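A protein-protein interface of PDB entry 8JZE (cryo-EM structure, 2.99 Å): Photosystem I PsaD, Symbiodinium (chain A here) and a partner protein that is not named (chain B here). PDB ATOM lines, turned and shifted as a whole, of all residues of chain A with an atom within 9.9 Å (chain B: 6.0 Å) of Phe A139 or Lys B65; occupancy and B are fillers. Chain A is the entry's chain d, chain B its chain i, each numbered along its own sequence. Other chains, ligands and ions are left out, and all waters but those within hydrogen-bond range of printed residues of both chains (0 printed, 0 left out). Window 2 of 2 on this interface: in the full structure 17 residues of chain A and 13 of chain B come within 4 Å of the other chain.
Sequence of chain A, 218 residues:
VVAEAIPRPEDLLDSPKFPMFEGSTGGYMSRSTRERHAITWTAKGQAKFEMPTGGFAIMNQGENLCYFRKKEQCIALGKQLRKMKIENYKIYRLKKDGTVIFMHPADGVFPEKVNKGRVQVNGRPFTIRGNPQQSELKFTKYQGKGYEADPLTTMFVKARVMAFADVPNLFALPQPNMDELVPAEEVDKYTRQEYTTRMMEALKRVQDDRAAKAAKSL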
ATOM      1  N   GLN A 133      14.212 -11.115  11.182  1.00  0.00           N
ATOM      2  CA  GLN A 133      12.929 -11.122  10.494  1.00  0.00           C
ATOM      3  C   GLN A 133      12.613  -9.734   9.952  1.00  0.00           C
ATOM      4  O   GLN A 133      12.896  -8.719  10.595  1.00  0.00           O
ATOM      5  CB  GLN A 133      11.820 -11.579  11.442  1.00  0.00           C
ATOM      6  CG  GLN A 133      12.175 -12.800  12.280  1.00  0.00           C
ATOM      7  CD  GLN A 133      11.051 -13.219  13.208  1.00  0.00           C
ATOM      8  OE1 GLN A 133       9.944 -12.685  13.143  1.00  0.00           O
ATOM      9  NE2 GLN A 133      11.330 -14.179  14.080  1.00  0.00           N
ATOM     10  N   GLN A 134      12.031  -9.691   8.750  1.00  0.00           N
ATOM     11  CA  GLN A 134      11.630  -8.412   8.170  1.00  0.00           C
ATOM     12  C   GLN A 134      10.583  -7.714   9.025  1.00  0.00           C
ATOM     13  O   GLN A 134      10.573  -6.482   9.111  1.00  0.00           O
ATOM     14  CB  GLN A 134      11.091  -8.609   6.751  1.00  0.00           C
ATOM     15  CG  GLN A 134      12.154  -8.726   5.673  1.00  0.00           C
ATOM     16  CD  GLN A 134      11.575  -8.587   4.277  1.00  0.00           C
ATOM     17  OE1 GLN A 134      10.366  -8.425   4.108  1.00  0.00           O
ATOM     18  NE2 GLN A 134      12.438  -8.641   3.269  1.00  0.00           N
ATOM     19  N   SER A 135       9.695  -8.482   9.658  1.00  0.00           N
ATOM     20  CA  SER A 135       8.636  -7.888  10.466  1.00  0.00           C
ATOM     21  C   SER A 135       9.193  -7.122  11.656  1.00  0.00           C
ATOM     22  O   SER A 135       8.560  -6.176  12.136  1.00  0.00           O
ATOM     23  CB  SER A 135       7.675  -8.973  10.944  1.00  0.00           C
ATOM     24  OG  SER A 135       7.240  -9.778   9.864  1.00  0.00           O
ATOM     25  N   GLU A 136      10.369  -7.512  12.144  1.00  0.00           N
ATOM     26  CA  GLU A 136      10.912  -6.877  13.337  1.00  0.00           C
ATOM     27  C   GLU A 136      11.459  -5.487  13.042  1.00  0.00           C
ATOM     28  O   GLU A 136      11.448  -4.619  13.922  1.00  0.00           O
ATOM     29  CB  GLU A 136      12.005  -7.754  13.943  1.00  0.00           C
ATOM     30  CG  GLU A 136      12.237  -7.497  15.413  1.00  0.00           C
ATOM     31  CD  GLU A 136      11.080  -7.966  16.261  1.00  0.00           C
ATOM     32  OE1 GLU A 136      10.771  -9.174  16.223  1.00  0.00           O
ATOM     33  OE2 GLU A 136      10.468  -7.126  16.953  1.00  0.00           O
ATOM     34  N   LEU A 137      11.932  -5.251  11.819  1.00  0.00           N
ATOM     35  CA  LEU A 137      12.617  -4.014  11.466  1.00  0.00           C
ATOM     36  C   LEU A 137      11.718  -3.042  10.709  1.00  0.00           C
ATOM     37  O   LEU A 137      12.205  -2.270   9.876  1.00  0.00           O
ATOM     38  CB  LEU A 137      13.869  -4.326  10.646  1.00  0.00           C
ATOM     39  CG  LEU A 137      14.843  -5.348  11.237  1.00  0.00           C
ATOM     40  CD1 LEU A 137      15.920  -5.708  10.233  1.00  0.00           C
ATOM     41  CD2 LEU A 137      15.469  -4.822  12.514  1.00  0.00           C
ATOM     42  N   LYS A 138      10.415  -3.056  10.982  1.00  0.00           N
ATOM     43  CA  LYS A 138       9.500  -2.165  10.281  1.00  0.00           C
ATOM     44  C   LYS A 138       9.749  -0.716  10.684  1.00  0.00           C
ATOM     45  O   LYS A 138       9.876  -0.402  11.872  1.00  0.00           O
ATOM     46  CB  LYS A 138       8.048  -2.547  10.569  1.00  0.00           C
ATOM     47  CG  LYS A 138       7.637  -3.901  10.022  1.00  0.00           C
ATOM     48  CD  LYS A 138       6.124  -4.022   9.921  1.00  0.00           C
ATOM     49  CE  LYS A 138       5.561  -3.045   8.900  1.00  0.00           C
ATOM     50  NZ  LYS A 138       6.125  -3.283   7.542  1.00  0.00           N
ATOM     51  N   PHE A 139       9.832   0.160   9.683  1.00  0.00           N
ATOM     52  CA  PHE A 139       9.972   1.603   9.858  1.00  0.00           C
ATOM     53  C   PHE A 139      11.258   1.985  10.587  1.00  0.00           C
ATOM     54  O   PHE A 139      11.350   3.075  11.159  1.00  0.00           O
ATOM     55  CB  PHE A 139       8.746   2.190  10.563  1.00  0.00           C
ATOM     56  CG  PHE A 139       7.447   1.825   9.901  1.00  0.00           C
ATOM     57  CD1 PHE A 139       7.152   2.287   8.629  1.00  0.00           C
ATOM     58  CD2 PHE A 139       6.529   1.011  10.542  1.00  0.00           C
ATOM     59  CE1 PHE A 139       5.965   1.949   8.010  1.00  0.00           C
ATOM     60  CE2 PHE A 139       5.339   0.670   9.930  1.00  0.00           C
ATOM     61  CZ  PHE A 139       5.056   1.140   8.663  1.00  0.00           C
ATOM     62  N   THR A 140      12.250   1.102  10.570  1.00  0.00           N
ATOM     63  CA  THR A 140      13.597   1.377  11.035  1.00  0.00           C
ATOM     64  C   THR A 140      14.500   1.625   9.827  1.00  0.00           C
ATOM     65  O   THR A 140      14.029   1.793   8.698  1.00  0.00           O
ATOM     66  CB  THR A 140      14.106   0.228  11.905  1.00  0.00           C
ATOM     67  OG1 THR A 140      14.051  -0.995  11.163  1.00  0.00           O
ATOM     68  CG2 THR A 140      13.254   0.092  13.152  1.00  0.00           C
ATOM     69  N   LYS A 141      15.815   1.668  10.061  1.00  0.00           N
ATOM     70  CA  LYS A 141      16.765   1.827   8.963  1.00  0.00           C
ATOM     71  C   LYS A 141      16.661   0.705   7.938  1.00  0.00           C
ATOM     72  O   LYS A 141      17.061   0.893   6.784  1.00  0.00           O
ATOM     73  CB  LYS A 141      18.197   1.879   9.502  1.00  0.00           C
ATOM     74  CG  LYS A 141      18.451   2.934  10.562  1.00  0.00           C
ATOM     75  CD  LYS A 141      19.759   2.665  11.297  1.00  0.00           C
ATOM     76  CE  LYS A 141      20.910   2.472  10.322  1.00  0.00           C
ATOM     77  NZ  LYS A 141      22.199   2.185  11.011  1.00  0.00           N
ATOM     78  N   TYR A 142      16.117  -0.447   8.328  1.00  0.00           N
ATOM     79  CA  TYR A 142      16.092  -1.634   7.483  1.00  0.00           C
ATOM     80  C   TYR A 142      14.653  -2.053   7.199  1.00  0.00           C
ATOM     81  O   TYR A 142      14.296  -3.221   7.376  1.00  0.00           O
ATOM     82  CB  TYR A 142      16.864  -2.776   8.150  1.00  0.00           C
ATOM     83  CG  TYR A 142      18.191  -2.354   8.744  1.00  0.00           C
ATOM     84  CD1 TYR A 142      19.234  -1.935   7.930  1.00  0.00           C
ATOM     85  CD2 TYR A 142      18.402  -2.381  10.117  1.00  0.00           C
ATOM     86  CE1 TYR A 142      20.446  -1.551   8.464  1.00  0.00           C
ATOM     87  CE2 TYR A 142      19.613  -2.000  10.661  1.00  0.00           C
ATOM     88  CZ  TYR A 142      20.631  -1.585   9.828  1.00  0.00           C
ATOM     89  OH  TYR A 142      21.838  -1.203  10.361  1.00  0.00           O
ATOM     90  N   GLN A 143      13.828  -1.092   6.770  1.00  0.00           N
ATOM     91  CA  GLN A 143      12.381  -1.288   6.684  1.00  0.00           C
ATOM     92  C   GLN A 143      12.018  -2.544   5.898  1.00  0.00           C
ATOM     93  O   GLN A 143      11.241  -3.382   6.368  1.00  0.00           O
ATOM     94  CB  GLN A 143      11.738  -0.049   6.055  1.00  0.00           C
ATOM     95  CG  GLN A 143      10.285   0.181   6.436  1.00  0.00           C
ATOM     96  CD  GLN A 143       9.312  -0.450   5.464  1.00  0.00           C
ATOM     97  OE1 GLN A 143       9.698  -0.891   4.382  1.00  0.00           O
ATOM     98  NE2 GLN A 143       8.042  -0.494   5.842  1.00  0.00           N
ATOM     99  N   GLY A 144      12.576  -2.697   4.702  1.00  0.00           N
ATOM    100  CA  GLY A 144      12.323  -3.883   3.908  1.00  0.00           C
ATOM    101  C   GLY A 144      13.601  -4.576   3.486  1.00  0.00           C
ATOM    102  O   GLY A 144      13.641  -5.251   2.453  1.00  0.00           O
ATOM    103  N   LYS A 145      14.653  -4.415   4.284  1.00  0.00           N
ATOM    104  CA  LYS A 145      16.004  -4.861   3.951  1.00  0.00           C
ATOM    105  C   LYS A 145      16.639  -5.577   5.137  1.00  0.00           C
ATOM    106  O   LYS A 145      17.742  -5.249   5.579  1.00  0.00           O
ATOM    107  CB  LYS A 145      16.849  -3.682   3.482  1.00  0.00           C
ATOM    108  CG  LYS A 145      16.366  -3.098   2.163  1.00  0.00           C
ATOM    109  CD  LYS A 145      17.070  -1.805   1.809  1.00  0.00           C
ATOM    110  CE  LYS A 145      16.574  -1.277   0.474  1.00  0.00           C
ATOM    111  NZ  LYS A 145      16.642  -2.324  -0.581  1.00  0.00           N
ATOM    112  N   ASP A 150      23.074  -4.821  10.567  1.00  0.00           N
ATOM    113  CA  ASP A 150      24.330  -5.121  11.228  1.00  0.00           C
ATOM    114  C   ASP A 150      24.114  -6.216  12.271  1.00  0.00           C
ATOM    115  O   ASP A 150      23.025  -6.332  12.837  1.00  0.00           O
ATOM    116  CB  ASP A 150      24.901  -3.868  11.888  1.00  0.00           C
ATOM    117  CG  ASP A 150      23.941  -3.237  12.877  1.00  0.00           C
ATOM    118  OD1 ASP A 150      23.821  -3.753  14.008  1.00  0.00           O
ATOM    119  OD2 ASP A 150      23.307  -2.223  12.520  1.00  0.00           O
ATOM    120  N   THR A 153      22.308  -5.358  15.512  1.00  0.00           N
ATOM    121  CA  THR A 153      20.859  -5.216  15.406  1.00  0.00           C
ATOM    122  C   THR A 153      20.176  -6.575  15.332  1.00  0.00           C
ATOM    123  O   THR A 153      19.089  -6.762  15.894  1.00  0.00           O
ATOM    124  CB  THR A 153      20.494  -4.368  14.188  1.00  0.00           C
ATOM    125  OG1 THR A 153      21.271  -4.786  13.060  1.00  0.00           O
ATOM    126  CG2 THR A 153      20.747  -2.896  14.464  1.00  0.00           C
ATOM    127  N   VAL A 157      17.354  -7.713  18.036  1.00  0.00           N
ATOM    128  CA  VAL A 157      15.999  -8.142  17.710  1.00  0.00           C
ATOM    129  C   VAL A 157      15.782  -9.599  18.102  1.00  0.00           C
ATOM    130  O   VAL A 157      14.666  -9.989  18.453  1.00  0.00           O
ATOM    131  CB  VAL A 157      15.684  -7.892  16.223  1.00  0.00           C
ATOM    132  CG1 VAL A 157      15.847  -6.421  15.885  1.00  0.00           C
ATOM    133  CG2 VAL A 157      16.552  -8.743  15.332  1.00  0.00           C
ATOM    134  N   ARG A 160      14.995  -9.434  21.674  1.00  0.00           N
ATOM    135  CA  ARG A 160      13.630  -8.934  21.805  1.00  0.00           C
ATOM    136  C   ARG A 160      12.609 -10.028  21.524  1.00  0.00           C
ATOM    137  O   ARG A 160      11.575 -10.108  22.193  1.00  0.00           O
ATOM    138  CB  ARG A 160      13.411  -7.748  20.870  1.00  0.00           C
ATOM    139  CG  ARG A 160      12.024  -7.142  20.967  1.00  0.00           C
ATOM    140  CD  ARG A 160      11.713  -6.302  19.746  1.00  0.00           C
ATOM    141  NE  ARG A 160      12.739  -5.298  19.498  1.00  0.00           N
ATOM    142  CZ  ARG A 160      12.846  -4.601  18.377  1.00  0.00           C
ATOM    143  NH1 ARG A 160      12.006  -4.776  17.370  1.00  0.00           N
ATOM    144  NH2 ARG A 160      13.825  -3.708  18.259  1.00  0.00           N
ATOM    145  N   ARG B  56      12.832  13.661  10.468  1.00  0.00           N
ATOM    146  CA  ARG B  56      13.881  13.598  11.482  1.00  0.00           C
ATOM    147  C   ARG B  56      13.940  14.870  12.321  1.00  0.00           C
ATOM    148  O   ARG B  56      14.398  14.831  13.468  1.00  0.00           O
ATOM    149  CB  ARG B  56      15.237  13.331  10.827  1.00  0.00           C
ATOM    150  CG  ARG B  56      15.342  11.993  10.096  1.00  0.00           C
ATOM    151  CD  ARG B  56      15.375  10.798  11.044  1.00  0.00           C
ATOM    152  NE  ARG B  56      14.061  10.453  11.574  1.00  0.00           N
ATOM    153  CZ  ARG B  56      13.141   9.767  10.911  1.00  0.00           C
ATOM    154  NH1 ARG B  56      13.351   9.346   9.674  1.00  0.00           N
ATOM    155  NH2 ARG B  56      11.980   9.499  11.501  1.00  0.00           N
ATOM    156  N   PHE B  61      10.219  12.118  16.324  1.00  0.00           N
ATOM    157  CA  PHE B  61      10.761  11.164  15.364  1.00  0.00           C
ATOM    158  C   PHE B  61      12.252  11.363  15.114  1.00  0.00           C
ATOM    159  O   PHE B  61      12.758  10.968  14.058  1.00  0.00           O
ATOM    160  CB  PHE B  61       9.989  11.247  14.048  1.00  0.00           C
ATOM    161  CG  PHE B  61       8.513  11.012  14.195  1.00  0.00           C
ATOM    162  CD1 PHE B  61       7.991   9.732  14.111  1.00  0.00           C
ATOM    163  CD2 PHE B  61       7.648  12.072  14.414  1.00  0.00           C
ATOM    164  CE1 PHE B  61       6.633   9.512  14.245  1.00  0.00           C
ATOM    165  CE2 PHE B  61       6.290  11.860  14.550  1.00  0.00           C
ATOM    166  CZ  PHE B  61       5.781  10.578  14.465  1.00  0.00           C
ATOM    167  N   ALA B  62      12.966  11.974  16.060  1.00  0.00           N
ATOM    168  CA  ALA B  62      14.407  12.145  15.905  1.00  0.00           C
ATOM    169  C   ALA B  62      15.110  10.794  15.835  1.00  0.00           C
ATOM    170  O   ALA B  62      15.703  10.436  14.813  1.00  0.00           O
ATOM    171  CB  ALA B  62      14.963  12.990  17.052  1.00  0.00           C
ATOM    172  N   ASN B  63      15.051  10.029  16.920  1.00  0.00           N
ATOM    173  CA  ASN B  63      15.630   8.686  16.958  1.00  0.00           C
ATOM    174  C   ASN B  63      14.553   7.630  16.714  1.00  0.00           C
ATOM    175  O   ASN B  63      14.313   6.743  17.531  1.00  0.00           O
ATOM    176  CB  ASN B  63      16.343   8.455  18.287  1.00  0.00           C
ATOM    177  CG  ASN B  63      17.643   9.229  18.395  1.00  0.00           C
ATOM    178  OD1 ASN B  63      17.660  10.377  18.838  1.00  0.00           O
ATOM    179  ND2 ASN B  63      18.741   8.599  17.993  1.00  0.00           N
ATOM    180  N   SER B  64      13.895   7.739  15.561  1.00  0.00           N
ATOM    181  CA  SER B  64      12.866   6.778  15.185  1.00  0.00           C
ATOM    182  C   SER B  64      13.405   5.649  14.321  1.00  0.00           C
ATOM    183  O   SER B  64      12.925   4.515  14.427  1.00  0.00           O
ATOM    184  CB  SER B  64      11.727   7.482  14.443  1.00  0.00           C
ATOM    185  OG  SER B  64      10.776   6.549  13.960  1.00  0.00           O
ATOM    186  N   LYS B  65      14.395   5.929  13.474  1.00  0.00           N
ATOM    187  CA  LYS B  65      14.936   4.906  12.592  1.00  0.00           C
ATOM    188  C   LYS B  65      15.900   3.965  13.297  1.00  0.00           C
ATOM    189  O   LYS B  65      16.198   2.895  12.757  1.00  0.00           O
ATOM    190  CB  LYS B  65      15.635   5.556  11.395  1.00  0.00           C
ATOM    191  CG  LYS B  65      14.675   6.218  10.427  1.00  0.00           C
ATOM    192  CD  LYS B  65      13.575   5.250  10.032  1.00  0.00           C
ATOM    193  CE  LYS B  65      12.343   5.975   9.527  1.00  0.00           C
ATOM    194  NZ  LYS B  65      11.190   5.046   9.380  1.00  0.00           N
ATOM    195  N   ASP B  66      16.378   4.322  14.480  1.00  0.00           N
ATOM    196  CA  ASP B  66      17.342   3.485  15.185  1.00  0.00           C
ATOM    197  C   ASP B  66      16.664   2.209  15.663  1.00  0.00           C
ATOM    198  O   ASP B  66      15.703   2.284  16.442  1.00  0.00           O
ATOM    199  CB  ASP B  66      17.938   4.246  16.367  1.00  0.00           C
ATOM    200  CG  ASP B  66      19.101   3.512  17.010  1.00  0.00           C
ATOM    201  OD1 ASP B  66      19.629   2.562  16.394  1.00  0.00           O
ATOM    202  OD2 ASP B  66      19.486   3.887  18.136  1.00  0.00           O
ATOM    203  N   PRO B  67      17.113   1.029  15.229  1.00  0.00           N
ATOM    204  CA  PRO B  67      16.499  -0.214  15.720  1.00  0.00           C
ATOM    205  C   PRO B  67      16.669  -0.422  17.213  1.00  0.00           C
ATOM    206  O   PRO B  67      15.878  -1.160  17.813  1.00  0.00           O
ATOM    207  CB  PRO B  67      17.221  -1.305  14.917  1.00  0.00           C
ATOM    208  CG  PRO B  67      17.764  -0.601  13.713  1.00  0.00           C
ATOM    209  CD  PRO B  67      18.121   0.772  14.188  1.00  0.00           C
ATOM    210  N   LEU B  68      17.669   0.204  17.828  1.00  0.00           N
ATOM    211  CA  LEU B  68      17.926   0.065  19.255  1.00  0.00           C
ATOM    212  C   LEU B  68      17.239   1.135  20.091  1.00  0.00           C
ATOM    213  O   LEU B  68      17.461   1.184  21.305  1.00  0.00           O
ATOM    214  CB  LEU B  68      19.434   0.097  19.530  1.00  0.00           C
ATOM    215  CG  LEU B  68      20.233  -1.197  19.340  1.00  0.00           C
ATOM    216  CD1 LEU B  68      20.367  -1.559  17.872  1.00  0.00           C
ATOM    217  CD2 LEU B  68      21.603  -1.079  19.987  1.00  0.00           C
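The backbone carbonyl oxygen of Phe A139 lies within hydrogen-bond range of the side-chain amino group of Lys B65. The backbone carbonyl oxygen (O) of Lys B65 sits at hydrogen-bond distance from the backbone NH (N) of Lys A141 (3.0 Å). NH2 of Arg A160 is in hydrogen-bond range of O of Pro B67, at 3.3 Å.
N of Leu B68 sits close to OD1 of Asp B66 (3.4 Å). The side-chain carboxylate (OE2) of Glu A136 lies within salt-bridge range of the guanidinium group (NH1) of Arg A160 (2.8 Å). O of Leu A137 is in hydrogen-bond range of OG1 of Thr A140, 2.6 Å away. The side-chain hydroxyl (OH) of Tyr A142 lies within hydrogen-bond range of the side-chain amino group (NZ) of Lys A141 (3.5 Å). The side-chain carboxylate of Asp A150 sits at hydrogen-bond distance from the side-chain hydroxyl of Tyr A142 (2.8 Å). OD1 of Asp A150 is in hydrogen-bond range of N of Thr A153 (2.7 Å).
Among the printed residues, merely in contact across the chains: Phe A139 with Ser B64, Thr A140 with Lys B65, Lys A141 with Pro B67, Tyr A142 with Pro B67, Thr A153 with Pro B67 and Thr A153 with Leu B68.
Of chain A, only Phe A139 (2.7 Å), Thr A140 (3.5 Å) and Lys A141 (3.0 Å) come within 4 Å of Lys B65. Printed residues of chain A within 4 Å of Leu B68: Thr A153. Of the printed residues of chain B, Thr A153 touches Pro B67 (3.8 Å) and Leu B68 (3.7 Å). The nearest printed residue of chain B that does not touch Phe A139 is Asp B66 (6.2 Å). The nearest printed residue of chain B that does not touch Thr A153 is Asp B66 (5.9 Å).
Printed residues of chain A that touch a printed residue of chain B: Phe A139, Thr A140, Lys A141, Tyr A142, Thr A153 and Arg A160. Among the printed residues, 9 pairs touch across the chains.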
